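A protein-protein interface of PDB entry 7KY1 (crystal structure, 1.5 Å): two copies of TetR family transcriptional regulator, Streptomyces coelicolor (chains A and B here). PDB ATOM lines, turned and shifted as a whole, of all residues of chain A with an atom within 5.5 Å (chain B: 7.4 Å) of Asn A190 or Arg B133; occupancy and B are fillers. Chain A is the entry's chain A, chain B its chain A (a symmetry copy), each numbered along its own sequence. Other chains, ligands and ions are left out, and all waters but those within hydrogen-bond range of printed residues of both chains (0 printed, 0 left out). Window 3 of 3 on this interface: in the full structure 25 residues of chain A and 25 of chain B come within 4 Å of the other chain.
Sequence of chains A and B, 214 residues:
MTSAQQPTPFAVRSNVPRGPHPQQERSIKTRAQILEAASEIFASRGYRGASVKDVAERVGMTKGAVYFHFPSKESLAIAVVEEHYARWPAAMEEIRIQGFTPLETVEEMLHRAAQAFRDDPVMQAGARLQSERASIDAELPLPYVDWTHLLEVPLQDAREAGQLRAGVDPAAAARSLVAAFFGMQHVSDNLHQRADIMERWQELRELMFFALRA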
ATOM      1  N   GLN A 185      -9.702 -10.445 -14.375  1.00  0.00           N
ATOM      2  CA  GLN A 185     -10.933 -10.716 -15.110  1.00  0.00           C
ATOM      3  C   GLN A 185     -11.673 -11.887 -14.490  1.00  0.00           C
ATOM      4  O   GLN A 185     -12.909 -11.902 -14.467  1.00  0.00           O
ATOM      5  CB  GLN A 185     -10.638 -10.970 -16.603  1.00  0.00           C
ATOM      6  CG  GLN A 185      -9.912 -12.281 -16.934  1.00  0.00           C
ATOM      7  CD  GLN A 185     -10.834 -13.496 -16.952  1.00  0.00           C
ATOM      8  OE1 GLN A 185     -12.055 -13.371 -17.078  1.00  0.00           O
ATOM      9  NE2 GLN A 185     -10.251 -14.673 -16.814  1.00  0.00           N
ATOM     10  N   HIS A 186     -10.930 -12.842 -13.930  1.00  0.00           N
ATOM     11  CA  HIS A 186     -11.552 -14.005 -13.311  1.00  0.00           C
ATOM     12  C   HIS A 186     -12.306 -13.625 -12.037  1.00  0.00           C
ATOM     13  O   HIS A 186     -13.441 -14.069 -11.817  1.00  0.00           O
ATOM     14  CB  HIS A 186     -10.483 -15.053 -13.017  1.00  0.00           C
ATOM     15  CG  HIS A 186     -11.047 -16.378 -12.626  1.00  0.00           C
ATOM     16  ND1 HIS A 186     -11.505 -17.292 -13.550  1.00  0.00           N
ATOM     17  CD2 HIS A 186     -11.245 -16.935 -11.410  1.00  0.00           C
ATOM     18  CE1 HIS A 186     -11.940 -18.368 -12.918  1.00  0.00           C
ATOM     19  NE2 HIS A 186     -11.798 -18.174 -11.618  1.00  0.00           N
ATOM     20  N   VAL A 187     -11.690 -12.808 -11.182  1.00  0.00           N
ATOM     21  CA  VAL A 187     -12.383 -12.299 -10.001  1.00  0.00           C
ATOM     22  C   VAL A 187     -13.638 -11.543 -10.411  1.00  0.00           C
ATOM     23  O   VAL A 187     -14.714 -11.713  -9.825  1.00  0.00           O
ATOM     24  CB  VAL A 187     -11.449 -11.399  -9.168  1.00  0.00           C
ATOM     25  CG1 VAL A 187     -12.234 -10.708  -8.074  1.00  0.00           C
ATOM     26  CG2 VAL A 187     -10.303 -12.207  -8.549  1.00  0.00           C
ATOM     27  N   SER A 188     -13.512 -10.675 -11.413  1.00  0.00           N
ATOM     28  CA  SER A 188     -14.654  -9.898 -11.876  1.00  0.00           C
ATOM     29  C   SER A 188     -15.767 -10.806 -12.392  1.00  0.00           C
ATOM     30  O   SER A 188     -16.952 -10.562 -12.128  1.00  0.00           O
ATOM     31  CB  SER A 188     -14.182  -8.918 -12.953  1.00  0.00           C
ATOM     32  OG  SER A 188     -15.252  -8.143 -13.442  1.00  0.00           O
ATOM     33  N   ASP A 189     -15.410 -11.875 -13.111  1.00  0.00           N
ATOM     34  CA  ASP A 189     -16.436 -12.822 -13.553  1.00  0.00           C
ATOM     35  C   ASP A 189     -17.082 -13.529 -12.366  1.00  0.00           C
ATOM     36  O   ASP A 189     -18.314 -13.632 -12.285  1.00  0.00           O
ATOM     37  CB  ASP A 189     -15.842 -13.849 -14.513  1.00  0.00           C
ATOM     38  CG  ASP A 189     -16.914 -14.631 -15.250  1.00  0.00           C
ATOM     39  OD1 ASP A 189     -17.944 -14.023 -15.629  1.00  0.00           O
ATOM     40  OD2 ASP A 189     -16.730 -15.845 -15.448  1.00  0.00           O
ATOM     41  N   ASN A 190     -16.263 -14.031 -11.433  1.00  0.00           N
ATOM     42  CA  ASN A 190     -16.790 -14.828 -10.324  1.00  0.00           C
ATOM     43  C   ASN A 190     -17.734 -14.018  -9.453  1.00  0.00           C
ATOM     44  O   ASN A 190     -18.776 -14.521  -9.013  1.00  0.00           O
ATOM     45  CB  ASN A 190     -15.648 -15.373  -9.457  1.00  0.00           C
ATOM     46  CG  ASN A 190     -14.964 -16.576 -10.066  1.00  0.00           C
ATOM     47  OD1 ASN A 190     -15.175 -16.905 -11.238  1.00  0.00           O
ATOM     48  ND2 ASN A 190     -14.128 -17.249  -9.272  1.00  0.00           N
ATOM     49  N   LEU A 191     -17.374 -12.777  -9.166  1.00  0.00           N
ATOM     50  CA  LEU A 191     -18.132 -12.003  -8.192  1.00  0.00           C
ATOM     51  C   LEU A 191     -19.196 -11.125  -8.829  1.00  0.00           C
ATOM     52  O   LEU A 191     -20.224 -10.858  -8.194  1.00  0.00           O
ATOM     53  CB  LEU A 191     -17.199 -11.119  -7.358  1.00  0.00           C
ATOM     54  CG  LEU A 191     -16.151 -11.804  -6.480  1.00  0.00           C
ATOM     55  CD1 LEU A 191     -15.257 -10.769  -5.837  1.00  0.00           C
ATOM     56  CD2 LEU A 191     -16.823 -12.690  -5.419  1.00  0.00           C
ATOM     57  N   HIS A 192     -18.978 -10.670 -10.068  1.00  0.00           N
ATOM     58  CA  HIS A 192     -19.841  -9.651 -10.653  1.00  0.00           C
ATOM     59  C   HIS A 192     -20.212  -9.925 -12.105  1.00  0.00           C
ATOM     60  O   HIS A 192     -20.763  -9.029 -12.761  1.00  0.00           O
ATOM     61  CB  HIS A 192     -19.179  -8.264 -10.562  1.00  0.00           C
ATOM     62  CG  HIS A 192     -18.756  -7.877  -9.179  1.00  0.00           C
ATOM     63  ND1 HIS A 192     -19.660  -7.539  -8.191  1.00  0.00           N
ATOM     64  CD2 HIS A 192     -17.526  -7.754  -8.625  1.00  0.00           C
ATOM     65  CE1 HIS A 192     -19.002  -7.233  -7.087  1.00  0.00           C
ATOM     66  NE2 HIS A 192     -17.708  -7.359  -7.322  1.00  0.00           N
ATOM     67  N   GLN A 193     -19.923 -11.118 -12.637  1.00  0.00           N
ATOM     68  CA  GLN A 193     -20.226 -11.447 -14.038  1.00  0.00           C
ATOM     69  C   GLN A 193     -19.571 -10.438 -14.985  1.00  0.00           C
ATOM     70  O   GLN A 193     -20.119 -10.086 -16.035  1.00  0.00           O
ATOM     71  CB  GLN A 193     -21.741 -11.539 -14.273  1.00  0.00           C
ATOM     72  CG  GLN A 193     -22.455 -12.613 -13.435  1.00  0.00           C
ATOM     73  CD  GLN A 193     -22.589 -12.250 -11.963  1.00  0.00           C
ATOM     74  OE1 GLN A 193     -21.967 -12.870 -11.098  1.00  0.00           O
ATOM     75  NE2 GLN A 193     -23.405 -11.239 -11.672  1.00  0.00           N
ATOM     76  N   ALA B 127      -8.448 -23.563  -2.398  1.00  0.00           N
ATOM     77  CA  ALA B 127      -8.431 -22.974  -3.738  1.00  0.00           C
ATOM     78  C   ALA B 127      -8.979 -23.942  -4.776  1.00  0.00           C
ATOM     79  O   ALA B 127      -9.657 -23.520  -5.720  1.00  0.00           O
ATOM     80  CB  ALA B 127      -7.020 -22.532  -4.121  1.00  0.00           C
ATOM     81  N   ARG B 128      -8.696 -25.238  -4.629  1.00  0.00           N
ATOM     82  CA  ARG B 128      -9.223 -26.201  -5.594  1.00  0.00           C
ATOM     83  C   ARG B 128     -10.739 -26.279  -5.511  1.00  0.00           C
ATOM     84  O   ARG B 128     -11.414 -26.311  -6.544  1.00  0.00           O
ATOM     85  CB  ARG B 128      -8.595 -27.579  -5.386  1.00  0.00           C
ATOM     86  CG  ARG B 128      -8.946 -28.550  -6.524  1.00  0.00           C
ATOM     87  CD  ARG B 128      -8.051 -29.780  -6.532  1.00  0.00           C
ATOM     88  NE  ARG B 128      -8.349 -30.669  -7.658  1.00  0.00           N
ATOM     89  CZ  ARG B 128      -7.617 -31.731  -7.978  1.00  0.00           C
ATOM     90  NH1 ARG B 128      -6.539 -32.035  -7.265  1.00  0.00           N
ATOM     91  NH2 ARG B 128      -7.957 -32.489  -9.013  1.00  0.00           N
ATOM     92  N   LEU B 129     -11.291 -26.306  -4.290  1.00  0.00           N
ATOM     93  CA  LEU B 129     -12.742 -26.305  -4.139  1.00  0.00           C
ATOM     94  C   LEU B 129     -13.359 -25.038  -4.709  1.00  0.00           C
ATOM     95  O   LEU B 129     -14.396 -25.093  -5.378  1.00  0.00           O
ATOM     96  CB  LEU B 129     -13.130 -26.477  -2.671  1.00  0.00           C
ATOM     97  CG  LEU B 129     -12.805 -27.852  -2.097  1.00  0.00           C
ATOM     98  CD1 LEU B 129     -12.961 -27.805  -0.585  1.00  0.00           C
ATOM     99  CD2 LEU B 129     -13.703 -28.947  -2.693  1.00  0.00           C
ATOM    100  N   GLN B 130     -12.725 -23.887  -4.481  1.00  0.00           N
ATOM    101  CA  GLN B 130     -13.271 -22.652  -5.024  1.00  0.00           C
ATOM    102  C   GLN B 130     -13.201 -22.635  -6.548  1.00  0.00           C
ATOM    103  O   GLN B 130     -14.058 -22.030  -7.197  1.00  0.00           O
ATOM    104  CB  GLN B 130     -12.535 -21.447  -4.434  1.00  0.00           C
ATOM    105  CG  GLN B 130     -12.881 -21.140  -2.976  1.00  0.00           C
ATOM    106  CD  GLN B 130     -14.234 -20.482  -2.805  1.00  0.00           C
ATOM    107  OE1 GLN B 130     -15.198 -20.783  -3.513  1.00  0.00           O
ATOM    108  NE2 GLN B 130     -14.307 -19.574  -1.852  1.00  0.00           N
ATOM    109  N   SER B 131     -12.189 -23.273  -7.135  1.00  0.00           N
ATOM    110  CA  SER B 131     -12.142 -23.344  -8.589  1.00  0.00           C
ATOM    111  C   SER B 131     -13.209 -24.290  -9.125  1.00  0.00           C
ATOM    112  O   SER B 131     -13.698 -24.100 -10.247  1.00  0.00           O
ATOM    113  CB  SER B 131     -10.752 -23.774  -9.055  1.00  0.00           C
ATOM    114  OG  SER B 131     -10.498 -25.136  -8.743  1.00  0.00           O
ATOM    115  N   GLU B 132     -13.589 -25.311  -8.344  1.00  0.00           N
ATOM    116  CA  GLU B 132     -14.680 -26.216  -8.700  1.00  0.00           C
ATOM    117  C   GLU B 132     -16.028 -25.711  -8.198  1.00  0.00           C
ATOM    118  O   GLU B 132     -16.976 -26.492  -8.031  1.00  0.00           O
ATOM    119  CB  GLU B 132     -14.373 -27.625  -8.184  1.00  0.00           C
ATOM    120  CG  GLU B 132     -13.139 -28.221  -8.862  1.00  0.00           C
ATOM    121  CD  GLU B 132     -12.631 -29.490  -8.217  1.00  0.00           C
ATOM    122  OE1 GLU B 132     -13.287 -29.999  -7.282  1.00  0.00           O
ATOM    123  OE2 GLU B 132     -11.559 -29.973  -8.649  1.00  0.00           O
ATOM    124  N   ARG B 133     -16.125 -24.392  -8.015  1.00  0.00           N
ATOM    125  CA  ARG B 133     -17.256 -23.743  -7.363  1.00  0.00           C
ATOM    126  C   ARG B 133     -18.556 -23.961  -8.122  1.00  0.00           C
ATOM    127  O   ARG B 133     -19.608 -24.190  -7.514  1.00  0.00           O
ATOM    128  CB  ARG B 133     -16.925 -22.256  -7.250  1.00  0.00           C
ATOM    129  CG  ARG B 133     -17.988 -21.274  -6.869  1.00  0.00           C
ATOM    130  CD  ARG B 133     -17.308 -19.897  -6.800  1.00  0.00           C
ATOM    131  NE  ARG B 133     -18.106 -18.913  -6.082  1.00  0.00           N
ATOM    132  CZ  ARG B 133     -18.588 -17.798  -6.619  1.00  0.00           C
ATOM    133  NH1 ARG B 133     -18.349 -17.503  -7.895  1.00  0.00           N
ATOM    134  NH2 ARG B 133     -19.309 -16.969  -5.873  1.00  0.00           N
ATOM    135  N   ALA B 134     -18.506 -23.891  -9.452  1.00  0.00           N
ATOM    136  CA  ALA B 134     -19.724 -24.002 -10.243  1.00  0.00           C
ATOM    137  C   ALA B 134     -20.386 -25.370 -10.101  1.00  0.00           C
ATOM    138  O   ALA B 134     -21.606 -25.481 -10.267  1.00  0.00           O
ATOM    139  CB  ALA B 134     -19.422 -23.708 -11.711  1.00  0.00           C
ATOM    140  N   SER B 135     -19.621 -26.419  -9.787  1.00  0.00           N
ATOM    141  CA  SER B 135     -20.163 -27.772  -9.800  1.00  0.00           C
ATOM    142  C   SER B 135     -20.151 -28.436  -8.424  1.00  0.00           C
ATOM    143  O   SER B 135     -20.118 -29.666  -8.333  1.00  0.00           O
ATOM    144  CB  SER B 135     -19.421 -28.639 -10.816  1.00  0.00           C
ATOM    145  OG  SER B 135     -18.213 -29.151 -10.284  1.00  0.00           O
ATOM    146  N   ILE B 136     -20.187 -27.651  -7.344  1.00  0.00           N
ATOM    147  CA  ILE B 136     -20.425 -28.164  -5.993  1.00  0.00           C
ATOM    148  C   ILE B 136     -21.771 -27.626  -5.524  1.00  0.00           C
ATOM    149  O   ILE B 136     -21.968 -26.408  -5.440  1.00  0.00           O
ATOM    150  CB  ILE B 136     -19.308 -27.773  -5.009  1.00  0.00           C
ATOM    151  CG1 ILE B 136     -18.029 -28.553  -5.310  1.00  0.00           C
ATOM    152  CG2 ILE B 136     -19.757 -28.032  -3.569  1.00  0.00           C
ATOM    153  CD1 ILE B 136     -16.815 -28.049  -4.542  1.00  0.00           C
ATOM    154  N   ASP B 137     -22.694 -28.532  -5.202  1.00  0.00           N
ATOM    155  CA  ASP B 137     -24.084 -28.162  -4.947  1.00  0.00           C
ATOM    156  C   ASP B 137     -24.267 -27.642  -3.518  1.00  0.00           C
ATOM    157  O   ASP B 137     -24.977 -28.220  -2.697  1.00  0.00           O
ATOM    158  CB  ASP B 137     -24.990 -29.353  -5.228  1.00  0.00           C
ATOM    159  CG  ASP B 137     -26.455 -28.968  -5.314  1.00  0.00           C
ATOM    160  OD1 ASP B 137     -26.746 -27.755  -5.360  1.00  0.00           O
ATOM    161  OD2 ASP B 137     -27.310 -29.878  -5.343  1.00  0.00           O
ATOM    162  N   ALA B 138     -23.607 -26.521  -3.232  1.00  0.00           N
ATOM    163  CA  ALA B 138     -23.747 -25.852  -1.944  1.00  0.00           C
ATOM    164  C   ALA B 138     -23.136 -24.463  -2.042  1.00  0.00           C
ATOM    165  O   ALA B 138     -22.266 -24.214  -2.880  1.00  0.00           O
ATOM    166  CB  ALA B 138     -23.079 -26.645  -0.814  1.00  0.00           C
ATOM    167  N   LEU B 140     -20.687 -22.166  -1.161  1.00  0.00           N
ATOM    168  CA  LEU B 140     -19.382 -21.965  -0.564  1.00  0.00           C
ATOM    169  C   LEU B 140     -19.235 -20.501  -0.150  1.00  0.00           C
ATOM    170  O   LEU B 140     -19.988 -19.638  -0.609  1.00  0.00           O
ATOM    171  CB  LEU B 140     -18.280 -22.365  -1.548  1.00  0.00           C
ATOM    172  CG  LEU B 140     -18.238 -23.819  -2.012  1.00  0.00           C
ATOM    173  CD1 LEU B 140     -17.165 -24.009  -3.071  1.00  0.00           C
ATOM    174  CD2 LEU B 140     -18.005 -24.762  -0.844  1.00  0.00           C
ATOM    175  N   PRO B 141     -18.293 -20.197   0.744  1.00  0.00           N
ATOM    176  CA  PRO B 141     -18.005 -18.791   1.042  1.00  0.00           C
ATOM    177  C   PRO B 141     -17.603 -18.068  -0.233  1.00  0.00           C
ATOM    178  O   PRO B 141     -17.008 -18.657  -1.139  1.00  0.00           O
ATOM    179  CB  PRO B 141     -16.838 -18.870   2.030  1.00  0.00           C
ATOM    180  CG  PRO B 141     -16.981 -20.213   2.658  1.00  0.00           C
ATOM    181  CD  PRO B 141     -17.513 -21.111   1.593  1.00  0.00           C
ATOM    182  N   LEU B 142     -17.950 -16.792  -0.310  1.00  0.00           N
ATOM    183  CA  LEU B 142     -17.543 -15.997  -1.461  1.00  0.00           C
ATOM    184  C   LEU B 142     -16.022 -15.931  -1.522  1.00  0.00           C
ATOM    185  O   LEU B 142     -15.375 -15.684  -0.495  1.00  0.00           O
ATOM    186  CB  LEU B 142     -18.105 -14.579  -1.392  1.00  0.00           C
ATOM    187  CG  LEU B 142     -19.527 -14.290  -1.867  1.00  0.00           C
ATOM    188  CD1 LEU B 142     -19.731 -12.783  -1.893  1.00  0.00           C
ATOM    189  CD2 LEU B 142     -19.763 -14.891  -3.240  1.00  0.00           C
ATOM    190  N   PRO B 143     -15.421 -16.142  -2.684  1.00  0.00           N
ATOM    191  CA  PRO B 143     -13.970 -16.017  -2.803  1.00  0.00           C
ATOM    192  C   PRO B 143     -13.544 -14.554  -2.854  1.00  0.00           C
ATOM    193  O   PRO B 143     -14.353 -13.646  -3.038  1.00  0.00           O
ATOM    194  CB  PRO B 143     -13.670 -16.729  -4.125  1.00  0.00           C
ATOM    195  CG  PRO B 143     -14.928 -16.493  -4.925  1.00  0.00           C
ATOM    196  CD  PRO B 143     -16.063 -16.529  -3.955  1.00  0.00           C
ATOM    197  N   TYR B 144     -12.252 -14.353  -2.594  1.00  0.00           N
ATOM    198  CA  TYR B 144     -11.510 -13.097  -2.775  1.00  0.00           C
ATOM    199  C   TYR B 144     -11.871 -12.002  -1.788  1.00  0.00           C
ATOM    200  O   TYR B 144     -11.014 -11.175  -1.451  1.00  0.00           O
ATOM    201  CB  TYR B 144     -11.694 -12.556  -4.196  1.00  0.00           C
ATOM    202  CG  TYR B 144     -11.648 -13.629  -5.235  1.00  0.00           C
ATOM    203  CD1 TYR B 144     -10.524 -14.427  -5.380  1.00  0.00           C
ATOM    204  CD2 TYR B 144     -12.740 -13.865  -6.055  1.00  0.00           C
ATOM    205  CE1 TYR B 144     -10.482 -15.434  -6.335  1.00  0.00           C
ATOM    206  CE2 TYR B 144     -12.711 -14.860  -7.011  1.00  0.00           C
ATOM    207  CZ  TYR B 144     -11.584 -15.647  -7.139  1.00  0.00           C
ATOM    208  OH  TYR B 144     -11.570 -16.639  -8.096  1.00  0.00           O
ATOM    209  N   PHE B 182      -3.939 -13.981  -6.915  1.00  0.00           N
ATOM    210  CA  PHE B 182      -4.711 -15.156  -7.287  1.00  0.00           C
ATOM    211  C   PHE B 182      -4.327 -15.637  -8.682  1.00  0.00           C
ATOM    212  O   PHE B 182      -4.182 -16.849  -8.939  1.00  0.00           O
ATOM    213  CB  PHE B 182      -6.218 -14.862  -7.247  1.00  0.00           C
ATOM    214  CG  PHE B 182      -7.001 -15.873  -8.032  1.00  0.00           C
ATOM    215  CD1 PHE B 182      -7.278 -17.123  -7.491  1.00  0.00           C
ATOM    216  CD2 PHE B 182      -7.354 -15.625  -9.354  1.00  0.00           C
ATOM    217  CE1 PHE B 182      -7.935 -18.089  -8.242  1.00  0.00           C
ATOM    218  CE2 PHE B 182      -8.014 -16.578 -10.108  1.00  0.00           C
ATOM    219  CZ  PHE B 182      -8.301 -17.817  -9.551  1.00  0.00           C
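No position is printed for both chains.
Of the 7 pairs that touch across the chains among the printed residues, none has its exchanged pair printed and touching as well.
The side-chain amide oxygen (OD1) of Asn A190 lies close to the backbone carbonyl oxygen (O) of His A186, at 3.4 Å.
Hydrophobic or aromatic side chains of chain B that line the printed part of chain A: Tyr B144 and Phe B182.
Along chain B the printed residues that touch a printed residue of chain A span positions 133 to 182.
Along chain A the printed residues that touch a printed residue of chain B span positions 186 to 191.
Among the printed residues, no Asp or Glu carboxylate lies within 4 Å of a Lys or Arg side-chain nitrogen of the other chain.
OH of Tyr B144 touches CD2 of His A186, 3.3 Å away.
His A186 touches Phe B182.
CG1 of Val A187 touches CD2 of Tyr B144, at 3.8 Å.
Pro B143 touches Leu A191.
Tyr B144 touches Leu A191.
O of Asn A190 lies within hydrogen-bond range of NH1 of Arg B133 (3.2 Å).
OH of Tyr B144 is in hydrogen-bond range of ND2 of Asn A190 (2.9 Å).
Of chain B, only Arg B133 (3.2 Å) and Tyr B144 (2.9 Å) come within 4 Å of Asn A190.
Arg B133 touches just one residue of chain A: Asn A190 (3.2 Å).
Of the printed residues of chain A, Tyr B144 touches His A186 (3.3 Å), Val A187 (3.8 Å), Asn A190 (2.9 Å) and Leu A191 (3.996 Å).
Of the printed residues of chain B, Val A187 touches Tyr B144.
Leu B142 touches none of the printed residues of chain A.
Ser A188 touches none of the printed residues of chain B.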
